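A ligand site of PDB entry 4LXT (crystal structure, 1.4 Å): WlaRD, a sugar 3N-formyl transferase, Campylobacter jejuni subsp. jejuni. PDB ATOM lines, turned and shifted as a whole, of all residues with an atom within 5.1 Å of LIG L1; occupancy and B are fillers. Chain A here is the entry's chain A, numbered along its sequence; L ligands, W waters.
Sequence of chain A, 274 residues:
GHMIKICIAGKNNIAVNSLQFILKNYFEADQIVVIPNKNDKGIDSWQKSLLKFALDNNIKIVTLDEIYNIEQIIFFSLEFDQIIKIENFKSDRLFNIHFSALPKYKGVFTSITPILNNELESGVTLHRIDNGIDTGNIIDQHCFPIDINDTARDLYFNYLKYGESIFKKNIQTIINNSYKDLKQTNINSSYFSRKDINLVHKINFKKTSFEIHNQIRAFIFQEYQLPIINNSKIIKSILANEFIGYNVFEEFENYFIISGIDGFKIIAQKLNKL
An oxygen (O14) of LIG L1 lies within hydrogen-bond range of the backbone carbonyl oxygen (O) of Gly 107, at 2.7 Å.
The backbone NH (N) of Phe 80 lies within hydrogen-bond range of an oxygen (O12) of LIG L1 (3.3 Å).
The backbone carbonyl oxygen of Phe 80 sits at hydrogen-bond distance from an oxygen (O12) of LIG L1 (2.7 Å).
O6 of LIG L1 lies within salt-bridge range of NZ of Lys 11 (2.8 Å).
The side-chain amide oxygen (OE1) of Gln 225 lies within hydrogen-bond range of a nitrogen (N1) of LIG L1 (2.8 Å).
N of Phe 109 is in hydrogen-bond range of O9 of LIG L1, 2.8 Å away.
O4 of LIG L1 is in hydrogen-bond range of N of Ser 111 (3.1 Å).
O4 of LIG L1 lies within hydrogen-bond range of N of Thr 110 (3.3 Å).
N of Asp 134 lies within hydrogen-bond range of O1 of LG2 L2, at 2.9 Å.
OD1 of Asn 96 lies close to O7 of LG2 L2.
N3 of LIG L1 lies within hydrogen-bond range of O7 of LG2 L2, 2.9 Å away.
N of Gly 107 sits at hydrogen-bond distance from OD2 of Asp 134, at 2.8 Å.
The side-chain amide nitrogen (ND2) of Asn 37 lies within hydrogen-bond range of the backbone carbonyl oxygen (O) of Glu 79, 2.9 Å away.
ND2 of Asn 12 lies within hydrogen-bond range of OH of Tyr 156 (2.9 Å).
The side-chain carboxylate (OD1) of Asp 134 is in hydrogen-bond range of a ring nitrogen (ND1) of His 98 (3.1 Å).
The backbone NH (N) of His 98 is in hydrogen-bond range of the side-chain amide oxygen (OD1) of Asn 96 (3.5 Å).
C of Glu 79 touches O12 of LIG L1 (3.1 Å).
His 98 touches LIG L1.
Val 108 touches LIG L1 (CB to O9, 3.7 Å).
Ile 112 touches LIG L1.
Tyr 156 touches LIG L1.
Leu 199 touches LIG L1 (CD1 to O1, 3.4 Å).
Phe 221 touches LIG L1.
CB of Tyr 224 touches N1 of LIG L1, 3.2 Å away.
15 residues have an atom within 4 Å of LIG L1: Lys 11, Glu 79, Phe 80, His 98, Gly 107, Val 108, Phe 109, Thr 110, Ser 111, Ile 112, Tyr 156, Leu 199, Phe 221, Tyr 224 and Gln 225.
The nearest printed residue that does not touch LIG L1 is Asp 81 (4.2 Å).
Water W8 lies within hydrogen-bond range of an oxygen (O7) of LIG L1 and the side-chain amino group of Lys 11.
Water W3 lies within hydrogen-bond range of OH of Tyr 156 (2.6 Å), OE1 of Glu 79 (2.7 Å) and O6 of LIG L1 (2.7 Å).
Water W9 lies within hydrogen-bond range of OH of Tyr 224, O6 of LIG L1, ND2 of Asn 12 and NZ of Lys 11.
Water W4 lies within hydrogen-bond range of the side-chain carboxylate (OE1) of Glu 79 (2.8 Å), an oxygen (O11) of LIG L1 (3.0 Å) and the side-chain hydroxyl (OG1) of Thr 110 (3.4 Å).
Water W1 lies within hydrogen-bond range of OE2 of Glu 79 (2.7 Å), N3 of LIG L1 (3.0 Å) and ND1 of His 98 (3.4 Å).
Water W10 bridges the side-chain amide oxygen of Gln 225 and an oxygen (O1) of LIG L1.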
ATOM      1  N   LYS A  11     -26.579  -2.895 -11.405  1.00  0.00           N
ATOM      2  CA  LYS A  11     -25.494  -1.970 -11.026  1.00  0.00           C
ATOM      3  C   LYS A  11     -25.127  -1.028 -12.118  1.00  0.00           C
ATOM      4  O   LYS A  11     -25.540  -1.155 -13.282  1.00  0.00           O
ATOM      5  CB  LYS A  11     -24.230  -2.730 -10.584  1.00  0.00           C
ATOM      6  CG  LYS A  11     -23.518  -3.439 -11.785  1.00  0.00           C
ATOM      7  CD  LYS A  11     -22.154  -3.949 -11.315  1.00  0.00           C
ATOM      8  CE  LYS A  11     -21.588  -4.774 -12.448  1.00  0.00           C
ATOM      9  NZ  LYS A  11     -20.181  -5.275 -12.077  1.00  0.00           N
ATOM     10  N   ASN A  12     -24.299  -0.062 -11.700  1.00  0.00           N
ATOM     11  CA  ASN A  12     -23.578   0.865 -12.604  1.00  0.00           C
ATOM     12  C   ASN A  12     -24.484   1.916 -13.253  1.00  0.00           C
ATOM     13  O   ASN A  12     -25.685   1.971 -12.881  1.00  0.00           O
ATOM     14  CB  ASN A  12     -22.677   0.119 -13.618  1.00  0.00           C
ATOM     15  CG  ASN A  12     -21.502  -0.553 -12.914  1.00  0.00           C
ATOM     16  OD1 ASN A  12     -21.261  -0.352 -11.725  1.00  0.00           O
ATOM     17  ND2 ASN A  12     -20.745  -1.343 -13.682  1.00  0.00           N
ATOM     18  N   ASN A  37     -26.303  -5.292  -6.657  1.00  0.00           N
ATOM     19  CA  ASN A  37     -25.375  -6.419  -6.687  1.00  0.00           C
ATOM     20  C   ASN A  37     -24.686  -6.557  -5.338  1.00  0.00           C
ATOM     21  O   ASN A  37     -24.588  -5.608  -4.553  1.00  0.00           O
ATOM     22  CB  ASN A  37     -24.357  -6.257  -7.809  1.00  0.00           C
ATOM     23  CG  ASN A  37     -24.960  -6.563  -9.182  1.00  0.00           C
ATOM     24  OD1 ASN A  37     -26.171  -6.791  -9.291  1.00  0.00           O
ATOM     25  ND2 ASN A  37     -24.136  -6.612 -10.214  1.00  0.00           N
ATOM     26  N   GLU A  79     -27.306  -5.455 -15.592  1.00  0.00           N
ATOM     27  CA  GLU A  79     -26.011  -5.903 -15.059  1.00  0.00           C
ATOM     28  C   GLU A  79     -26.143  -6.551 -13.693  1.00  0.00           C
ATOM     29  O   GLU A  79     -25.249  -6.472 -12.834  1.00  0.00           O
ATOM     30  CB  GLU A  79     -24.975  -4.752 -15.087  1.00  0.00           C
ATOM     31  CG  GLU A  79     -24.710  -4.227 -16.496  1.00  0.00           C
ATOM     32  CD  GLU A  79     -24.368  -5.390 -17.482  1.00  0.00           C
ATOM     33  OE1 GLU A  79     -23.247  -5.993 -17.440  1.00  0.00           O
ATOM     34  OE2 GLU A  79     -25.205  -5.755 -18.382  1.00  0.00           O
ATOM     35  N   PHE A  80     -27.261  -7.271 -13.453  1.00  0.00           N
ATOM     36  CA  PHE A  80     -27.466  -8.015 -12.207  1.00  0.00           C
ATOM     37  C   PHE A  80     -26.565  -9.242 -12.113  1.00  0.00           C
ATOM     38  O   PHE A  80     -26.294  -9.916 -13.129  1.00  0.00           O
ATOM     39  CB  PHE A  80     -28.948  -8.432 -12.147  1.00  0.00           C
ATOM     40  CG  PHE A  80     -29.424  -8.977 -10.858  1.00  0.00           C
ATOM     41  CD1 PHE A  80     -30.244 -10.116 -10.871  1.00  0.00           C
ATOM     42  CD2 PHE A  80     -29.106  -8.374  -9.647  1.00  0.00           C
ATOM     43  CE1 PHE A  80     -30.762 -10.623  -9.682  1.00  0.00           C
ATOM     44  CE2 PHE A  80     -29.574  -8.900  -8.450  1.00  0.00           C
ATOM     45  CZ  PHE A  80     -30.428 -10.008  -8.481  1.00  0.00           C
ATOM     46  N   ASP A  81     -26.145  -9.539 -10.892  1.00  0.00           N
ATOM     47  CA  ASP A  81     -25.117 -10.543 -10.638  1.00  0.00           C
ATOM     48  C   ASP A  81     -25.661 -11.929 -10.337  1.00  0.00           C
ATOM     49  O   ASP A  81     -24.864 -12.861 -10.146  1.00  0.00           O
ATOM     50  CB  ASP A  81     -24.117 -10.105  -9.553  1.00  0.00           C
ATOM     51  CG  ASP A  81     -24.771  -9.853  -8.215  1.00  0.00           C
ATOM     52  OD1 ASP A  81     -24.017  -9.658  -7.221  1.00  0.00           O
ATOM     53  OD2 ASP A  81     -26.013  -9.829  -8.075  1.00  0.00           O
ATOM     54  N   ASN A  96     -34.194  -8.432 -19.230  1.00  0.00           N
ATOM     55  CA  ASN A  96     -32.747  -8.131 -19.027  1.00  0.00           C
ATOM     56  C   ASN A  96     -32.278  -7.380 -20.251  1.00  0.00           C
ATOM     57  O   ASN A  96     -32.782  -7.537 -21.359  1.00  0.00           O
ATOM     58  CB  ASN A  96     -31.989  -9.448 -18.968  1.00  0.00           C
ATOM     59  CG  ASN A  96     -30.483  -9.250 -18.811  1.00  0.00           C
ATOM     60  OD1 ASN A  96     -29.700  -9.661 -19.716  1.00  0.00           O
ATOM     61  ND2 ASN A  96     -30.081  -8.687 -17.721  1.00  0.00           N
ATOM     62  N   HIS A  98     -28.728  -7.354 -22.119  1.00  0.00           N
ATOM     63  CA  HIS A  98     -27.441  -8.048 -22.218  1.00  0.00           C
ATOM     64  C   HIS A  98     -26.518  -7.269 -23.125  1.00  0.00           C
ATOM     65  O   HIS A  98     -26.910  -6.833 -24.196  1.00  0.00           O
ATOM     66  CB  HIS A  98     -27.625  -9.482 -22.763  1.00  0.00           C
ATOM     67  CG  HIS A  98     -26.320 -10.219 -22.834  1.00  0.00           C
ATOM     68  ND1 HIS A  98     -25.646 -10.631 -21.706  1.00  0.00           N
ATOM     69  CD2 HIS A  98     -25.569 -10.604 -23.887  1.00  0.00           C
ATOM     70  CE1 HIS A  98     -24.530 -11.248 -22.075  1.00  0.00           C
ATOM     71  NE2 HIS A  98     -24.455 -11.232 -23.387  1.00  0.00           N
ATOM     72  N   GLY A 107     -23.038 -15.044 -21.815  1.00  0.00           N
ATOM     73  CA  GLY A 107     -22.136 -15.314 -20.691  1.00  0.00           C
ATOM     74  C   GLY A 107     -21.544 -14.018 -20.168  1.00  0.00           C
ATOM     75  O   GLY A 107     -22.302 -13.072 -19.902  1.00  0.00           O
ATOM     76  N   VAL A 108     -20.237 -14.001 -19.929  1.00  0.00           N
ATOM     77  CA  VAL A 108     -19.584 -12.932 -19.150  1.00  0.00           C
ATOM     78  C   VAL A 108     -18.462 -12.306 -19.982  1.00  0.00           C
ATOM     79  O   VAL A 108     -18.153 -12.736 -21.105  1.00  0.00           O
ATOM     80  CB  VAL A 108     -19.085 -13.430 -17.784  1.00  0.00           C
ATOM     81  CG1 VAL A 108     -20.285 -14.031 -16.997  1.00  0.00           C
ATOM     82  CG2 VAL A 108     -18.003 -14.450 -18.002  1.00  0.00           C
ATOM     83  N   PHE A 109     -17.890 -11.245 -19.392  1.00  0.00           N
ATOM     84  CA  PHE A 109     -16.723 -10.578 -20.024  1.00  0.00           C
ATOM     85  C   PHE A 109     -17.011 -10.109 -21.426  1.00  0.00           C
ATOM     86  O   PHE A 109     -16.134 -10.187 -22.331  1.00  0.00           O
ATOM     87  CB  PHE A 109     -15.441 -11.430 -19.981  1.00  0.00           C
ATOM     88  CG  PHE A 109     -14.964 -11.777 -18.621  1.00  0.00           C
ATOM     89  CD1 PHE A 109     -14.424 -13.014 -18.356  1.00  0.00           C
ATOM     90  CD2 PHE A 109     -15.053 -10.874 -17.570  1.00  0.00           C
ATOM     91  CE1 PHE A 109     -13.964 -13.358 -17.058  1.00  0.00           C
ATOM     92  CE2 PHE A 109     -14.621 -11.194 -16.279  1.00  0.00           C
ATOM     93  CZ  PHE A 109     -14.045 -12.442 -16.021  1.00  0.00           C
ATOM     94  N   THR A 110     -18.176  -9.548 -21.669  1.00  0.00           N
ATOM     95  CA  THR A 110     -18.560  -9.249 -22.997  1.00  0.00           C
ATOM     96  C   THR A 110     -17.958  -7.981 -23.616  1.00  0.00           C
ATOM     97  O   THR A 110     -18.171  -7.692 -24.785  1.00  0.00           O
ATOM     98  CB  THR A 110     -20.103  -9.191 -23.187  1.00  0.00           C
ATOM     99  OG1 THR A 110     -20.553  -7.986 -22.570  1.00  0.00           O
ATOM    100  CG2 THR A 110     -20.883 -10.398 -22.630  1.00  0.00           C
ATOM    101  N   SER A 111     -17.193  -7.220 -22.828  1.00  0.00           N
ATOM    102  CA  SER A 111     -16.311  -6.177 -23.366  1.00  0.00           C
ATOM    103  C   SER A 111     -14.983  -6.736 -23.837  1.00  0.00           C
ATOM    104  O   SER A 111     -14.292  -5.975 -24.547  1.00  0.00           O
ATOM    105  CB  SER A 111     -16.125  -5.051 -22.340  1.00  0.00           C
ATOM    106  OG  SER A 111     -17.374  -4.478 -21.945  1.00  0.00           O
ATOM    107  N   ILE A 112     -14.650  -7.958 -23.447  1.00  0.00           N
ATOM    108  CA  ILE A 112     -13.392  -8.616 -23.897  1.00  0.00           C
ATOM    109  C   ILE A 112     -13.710  -9.550 -25.074  1.00  0.00           C
ATOM    110  O   ILE A 112     -13.047  -9.515 -26.126  1.00  0.00           O
ATOM    111  CB  ILE A 112     -12.784  -9.385 -22.761  1.00  0.00           C
ATOM    112  CG1 ILE A 112     -12.454  -8.472 -21.567  1.00  0.00           C
ATOM    113  CG2 ILE A 112     -11.516 -10.195 -23.226  1.00  0.00           C
ATOM    114  CD1 ILE A 112     -11.889  -9.169 -20.373  1.00  0.00           C
ATOM    115  N   ASP A 134     -28.683 -15.746 -20.882  1.00  0.00           N
ATOM    116  CA  ASP A 134     -28.857 -14.918 -22.053  1.00  0.00           C
ATOM    117  C   ASP A 134     -29.525 -15.580 -23.247  1.00  0.00           C
ATOM    118  O   ASP A 134     -29.283 -15.216 -24.397  1.00  0.00           O
ATOM    119  CB  ASP A 134     -27.492 -14.324 -22.497  1.00  0.00           C
ATOM    120  CG  ASP A 134     -26.737 -13.693 -21.332  1.00  0.00           C
ATOM    121  OD1 ASP A 134     -27.361 -12.962 -20.523  1.00  0.00           O
ATOM    122  OD2 ASP A 134     -25.511 -13.907 -21.207  1.00  0.00           O
ATOM    123  N   TYR A 156     -17.155  -1.107 -23.209  1.00  0.00           N
ATOM    124  CA  TYR A 156     -18.026  -1.141 -22.032  1.00  0.00           C
ATOM    125  C   TYR A 156     -18.787   0.170 -21.913  1.00  0.00           C
ATOM    126  O   TYR A 156     -20.012   0.154 -21.644  1.00  0.00           O
ATOM    127  CB  TYR A 156     -17.254  -1.421 -20.738  1.00  0.00           C
ATOM    128  CG  TYR A 156     -18.191  -1.636 -19.582  1.00  0.00           C
ATOM    129  CD1 TYR A 156     -18.933  -2.810 -19.502  1.00  0.00           C
ATOM    130  CD2 TYR A 156     -18.318  -0.677 -18.585  1.00  0.00           C
ATOM    131  CE1 TYR A 156     -19.819  -3.031 -18.439  1.00  0.00           C
ATOM    132  CE2 TYR A 156     -19.198  -0.905 -17.511  1.00  0.00           C
ATOM    133  CZ  TYR A 156     -19.947  -2.045 -17.461  1.00  0.00           C
ATOM    134  OH  TYR A 156     -20.814  -2.245 -16.385  1.00  0.00           O
ATOM    135  N   LEU A 199      -7.585 -13.450 -17.341  1.00  0.00           N
ATOM    136  CA  LEU A 199      -7.529 -11.998 -17.296  1.00  0.00           C
ATOM    137  C   LEU A 199      -6.107 -11.416 -17.325  1.00  0.00           C
ATOM    138  O   LEU A 199      -5.960 -10.220 -17.519  1.00  0.00           O
ATOM    139  CB  LEU A 199      -8.350 -11.445 -16.115  1.00  0.00           C
ATOM    140  CG  LEU A 199      -9.865 -11.725 -16.234  1.00  0.00           C
ATOM    141  CD1 LEU A 199     -10.471 -11.472 -14.830  1.00  0.00           C
ATOM    142  CD2 LEU A 199     -10.504 -10.829 -17.260  1.00  0.00           C
ATOM    143  N   PHE A 221      -8.488  -2.308 -19.806  1.00  0.00           N
ATOM    144  CA  PHE A 221      -9.624  -1.756 -19.050  1.00  0.00           C
ATOM    145  C   PHE A 221      -9.015  -1.416 -17.687  1.00  0.00           C
ATOM    146  O   PHE A 221      -9.017  -2.213 -16.758  1.00  0.00           O
ATOM    147  CB  PHE A 221     -10.761  -2.807 -18.954  1.00  0.00           C
ATOM    148  CG  PHE A 221     -12.109  -2.224 -18.557  1.00  0.00           C
ATOM    149  CD1 PHE A 221     -13.268  -2.788 -19.122  1.00  0.00           C
ATOM    150  CD2 PHE A 221     -12.248  -1.179 -17.646  1.00  0.00           C
ATOM    151  CE1 PHE A 221     -14.518  -2.281 -18.759  1.00  0.00           C
ATOM    152  CE2 PHE A 221     -13.539  -0.695 -17.267  1.00  0.00           C
ATOM    153  CZ  PHE A 221     -14.663  -1.265 -17.862  1.00  0.00           C
ATOM    154  N   TYR A 224      -9.556  -2.405 -13.996  1.00  0.00           N
ATOM    155  CA  TYR A 224      -9.316  -3.797 -13.687  1.00  0.00           C
ATOM    156  C   TYR A 224      -7.867  -4.224 -13.997  1.00  0.00           C
ATOM    157  O   TYR A 224      -7.203  -4.695 -13.053  1.00  0.00           O
ATOM    158  CB  TYR A 224     -10.303  -4.666 -14.480  1.00  0.00           C
ATOM    159  CG  TYR A 224     -11.758  -4.454 -14.107  1.00  0.00           C
ATOM    160  CD1 TYR A 224     -12.231  -4.941 -12.894  1.00  0.00           C
ATOM    161  CD2 TYR A 224     -12.627  -3.764 -14.959  1.00  0.00           C
ATOM    162  CE1 TYR A 224     -13.577  -4.746 -12.525  1.00  0.00           C
ATOM    163  CE2 TYR A 224     -13.963  -3.569 -14.586  1.00  0.00           C
ATOM    164  CZ  TYR A 224     -14.390  -4.071 -13.405  1.00  0.00           C
ATOM    165  OH  TYR A 224     -15.740  -3.896 -13.028  1.00  0.00           O
ATOM    166  N   GLN A 225      -7.413  -4.129 -15.240  1.00  0.00           N
ATOM    167  CA  GLN A 225      -6.037  -4.599 -15.537  1.00  0.00           C
ATOM    168  C   GLN A 225      -5.667  -3.954 -16.846  1.00  0.00           C
ATOM    169  O   GLN A 225      -6.479  -3.403 -17.594  1.00  0.00           O
ATOM    170  CB  GLN A 225      -5.875  -6.110 -15.612  1.00  0.00           C
ATOM    171  CG  GLN A 225      -6.461  -6.792 -16.868  1.00  0.00           C
ATOM    172  CD  GLN A 225      -7.983  -6.830 -16.920  1.00  0.00           C
ATOM    173  OE1 GLN A 225      -8.631  -7.356 -16.010  1.00  0.00           O
ATOM    174  NE2 GLN A 225      -8.522  -6.246 -17.987  1.00  0.00           N
HETATM  175  O1  LIG L   1     -11.425  -8.393 -13.742  1.00  0.00           O
HETATM  176  C1  LIG L   1     -12.082  -7.857 -14.669  1.00  0.00           C
HETATM  177  N1  LIG L   1     -11.438  -7.412 -15.779  1.00  0.00           N
HETATM  178  C2  LIG L   1     -12.068  -6.786 -16.783  1.00  0.00           C
HETATM  179  O2  LIG L   1     -11.474  -6.378 -17.810  1.00  0.00           O
HETATM  180  C3  LIG L   1     -13.492  -7.655 -14.624  1.00  0.00           C
HETATM  181  C4  LIG L   1     -14.267  -8.136 -13.395  1.00  0.00           C
HETATM  182  C5  LIG L   1     -14.064  -7.056 -15.638  1.00  0.00           C
HETATM  183  N2  LIG L   1     -13.429  -6.616 -16.728  1.00  0.00           N
HETATM  184  C6  LIG L   1     -14.094  -5.922 -17.818  1.00  0.00           C
HETATM  185  O3  LIG L   1     -15.172  -5.122 -17.338  1.00  0.00           O
HETATM  186  C7  LIG L   1     -14.624  -6.770 -18.951  1.00  0.00           C
HETATM  187  C8  LIG L   1     -16.100  -6.889 -18.569  1.00  0.00           C
HETATM  188  O4  LIG L   1     -16.843  -7.209 -19.751  1.00  0.00           O
HETATM  189  C9  LIG L   1     -16.392  -5.521 -18.043  1.00  0.00           C
HETATM  190  C10 LIG L   1     -17.539  -5.482 -17.049  1.00  0.00           C
HETATM  191  O5  LIG L   1     -17.281  -6.454 -16.063  1.00  0.00           O
HETATM  192  P1  LIG L   1     -18.498  -6.898 -15.116  1.00  0.00           P
HETATM  193  O6  LIG L   1     -19.295  -5.692 -14.682  1.00  0.00           O
HETATM  194  O7  LIG L   1     -17.936  -7.760 -14.113  1.00  0.00           O
HETATM  195  O8  LIG L   1     -19.504  -7.700 -16.058  1.00  0.00           O
HETATM  196  P2  LIG L   1     -19.430  -8.671 -17.333  1.00  0.00           P
HETATM  197  O9  LIG L   1     -18.591  -9.838 -17.017  1.00  0.00           O
HETATM  198  O10 LIG L   1     -19.205  -7.919 -18.547  1.00  0.00           O
HETATM  199  O11 LIG L   1     -20.988  -9.128 -17.402  1.00  0.00           O
HETATM  200  O12 LIG L   1     -25.133  -8.911 -15.396  1.00  0.00           O
HETATM  201  C11 LIG L   1     -23.962  -9.733 -15.693  1.00  0.00           C
HETATM  202  C12 LIG L   1     -22.662  -9.165 -15.098  1.00  0.00           C
HETATM  203  O13 LIG L   1     -21.685 -10.167 -15.449  1.00  0.00           O
HETATM  204  C13 LIG L   1     -22.604  -9.033 -13.576  1.00  0.00           C
HETATM  205  C14 LIG L   1     -23.861  -9.665 -17.202  1.00  0.00           C
HETATM  206  N3  LIG L   1     -25.131 -10.016 -17.888  1.00  0.00           N
HETATM  207  C15 LIG L   1     -22.749 -10.662 -17.611  1.00  0.00           C
HETATM  208  O14 LIG L   1     -22.546 -10.529 -18.998  1.00  0.00           O
HETATM  209  C16 LIG L   1     -21.484 -10.325 -16.840  1.00  0.00           C
HETATM  210  N1  LG2 L   2     -30.962 -14.933 -14.873  1.00  0.00           N
HETATM  211  C1  LG2 L   2     -31.286 -15.781 -15.878  1.00  0.00           C
HETATM  212  N2  LG2 L   2     -31.969 -16.929 -15.605  1.00  0.00           N
HETATM  213  N3  LG2 L   2     -31.021 -15.559 -17.171  1.00  0.00           N
HETATM  214  C2  LG2 L   2     -30.314 -14.487 -17.557  1.00  0.00           C
HETATM  215  O1  LG2 L   2     -30.164 -14.357 -18.874  1.00  0.00           O
HETATM  216  C3  LG2 L   2     -29.932 -13.549 -16.600  1.00  0.00           C
HETATM  217  N4  LG2 L   2     -29.050 -12.460 -16.857  1.00  0.00           N
HETATM  218  C4  LG2 L   2     -28.348 -11.881 -15.677  1.00  0.00           C
HETATM  219  C5  LG2 L   2     -29.389 -11.672 -14.581  1.00  0.00           C
HETATM  220  N5  LG2 L   2     -29.932 -13.013 -14.253  1.00  0.00           N
HETATM  221  C6  LG2 L   2     -30.246 -13.856 -15.278  1.00  0.00           C
HETATM  222  C7  LG2 L   2     -27.296 -12.701 -14.909  1.00  0.00           C
HETATM  223  N6  LG2 L   2     -26.004 -12.738 -15.561  1.00  0.00           N
HETATM  224  C8  LG2 L   2     -23.088 -15.455 -14.281  1.00  0.00           C
HETATM  225  C9  LG2 L   2     -23.793 -14.664 -13.359  1.00  0.00           C
HETATM  226  C10 LG2 L   2     -24.766 -13.738 -13.797  1.00  0.00           C
HETATM  227  C11 LG2 L   2     -25.071 -13.611 -15.124  1.00  0.00           C
HETATM  228  C12 LG2 L   2     -24.387 -14.393 -16.049  1.00  0.00           C
HETATM  229  C13 LG2 L   2     -23.433 -15.296 -15.615  1.00  0.00           C
HETATM  230  C14 LG2 L   2     -22.102 -16.454 -13.759  1.00  0.00           C
HETATM  231  O2  LG2 L   2     -21.869 -16.579 -12.564  1.00  0.00           O
HETATM  232  N7  LG2 L   2     -21.555 -17.280 -14.675  1.00  0.00           N
HETATM  233  C15 LG2 L   2     -20.633 -18.358 -14.311  1.00  0.00           C
HETATM  234  C16 LG2 L   2     -21.278 -19.658 -14.864  1.00  0.00           C
HETATM  235  C17 LG2 L   2     -22.517 -20.068 -14.039  1.00  0.00           C
HETATM  236  C18 LG2 L   2     -23.098 -21.411 -14.442  1.00  0.00           C
HETATM  237  O3  LG2 L   2     -22.481 -22.174 -15.212  1.00  0.00           O
HETATM  238  O4  LG2 L   2     -24.212 -21.707 -13.912  1.00  0.00           O
HETATM  239  C19 LG2 L   2     -19.249 -18.229 -14.929  1.00  0.00           C
HETATM  240  O5  LG2 L   2     -19.126 -17.598 -16.001  1.00  0.00           O
HETATM  241  O6  LG2 L   2     -18.309 -18.803 -14.324  1.00  0.00           O
HETATM  242  C20 LG2 L   2     -28.651 -12.097 -18.017  1.00  0.00           C
HETATM  243  O7  LG2 L   2     -27.759 -11.222 -18.174  1.00  0.00           O
HETATM  244  O   HOH W   1     -24.655  -7.881 -20.004  1.00  0.00           O
HETATM  245  O   HOH W   2     -11.985 -10.184 -11.791  1.00  0.00           O
HETATM  246  O   HOH W   3     -21.453  -4.735 -15.925  1.00  0.00           O
HETATM  247  O   HOH W   4     -21.989  -7.289 -19.603  1.00  0.00           O
HETATM  248  O   HOH W   5     -25.087 -12.663 -18.796  1.00  0.00           O
HETATM  249  O   HOH W   6     -19.897 -11.350 -13.663  1.00  0.00           O
HETATM  250  O   HOH W   7     -17.526 -10.320 -14.624  1.00  0.00           O
HETATM  251  O   HOH W   8     -17.847  -7.644 -11.497  1.00  0.00           O
HETATM  252  O   HOH W   9     -18.393  -3.103 -13.790  1.00  0.00           O
HETATM  253  O   HOH W  10      -8.025  -8.495 -13.525  1.00  0.00           O
HETATM  254  O   HOH W  11     -27.245  -7.822 -17.622  1.00  0.00           O
HETATM  255  O   HOH W  12     -19.505  -6.008 -20.841  1.00  0.00           O
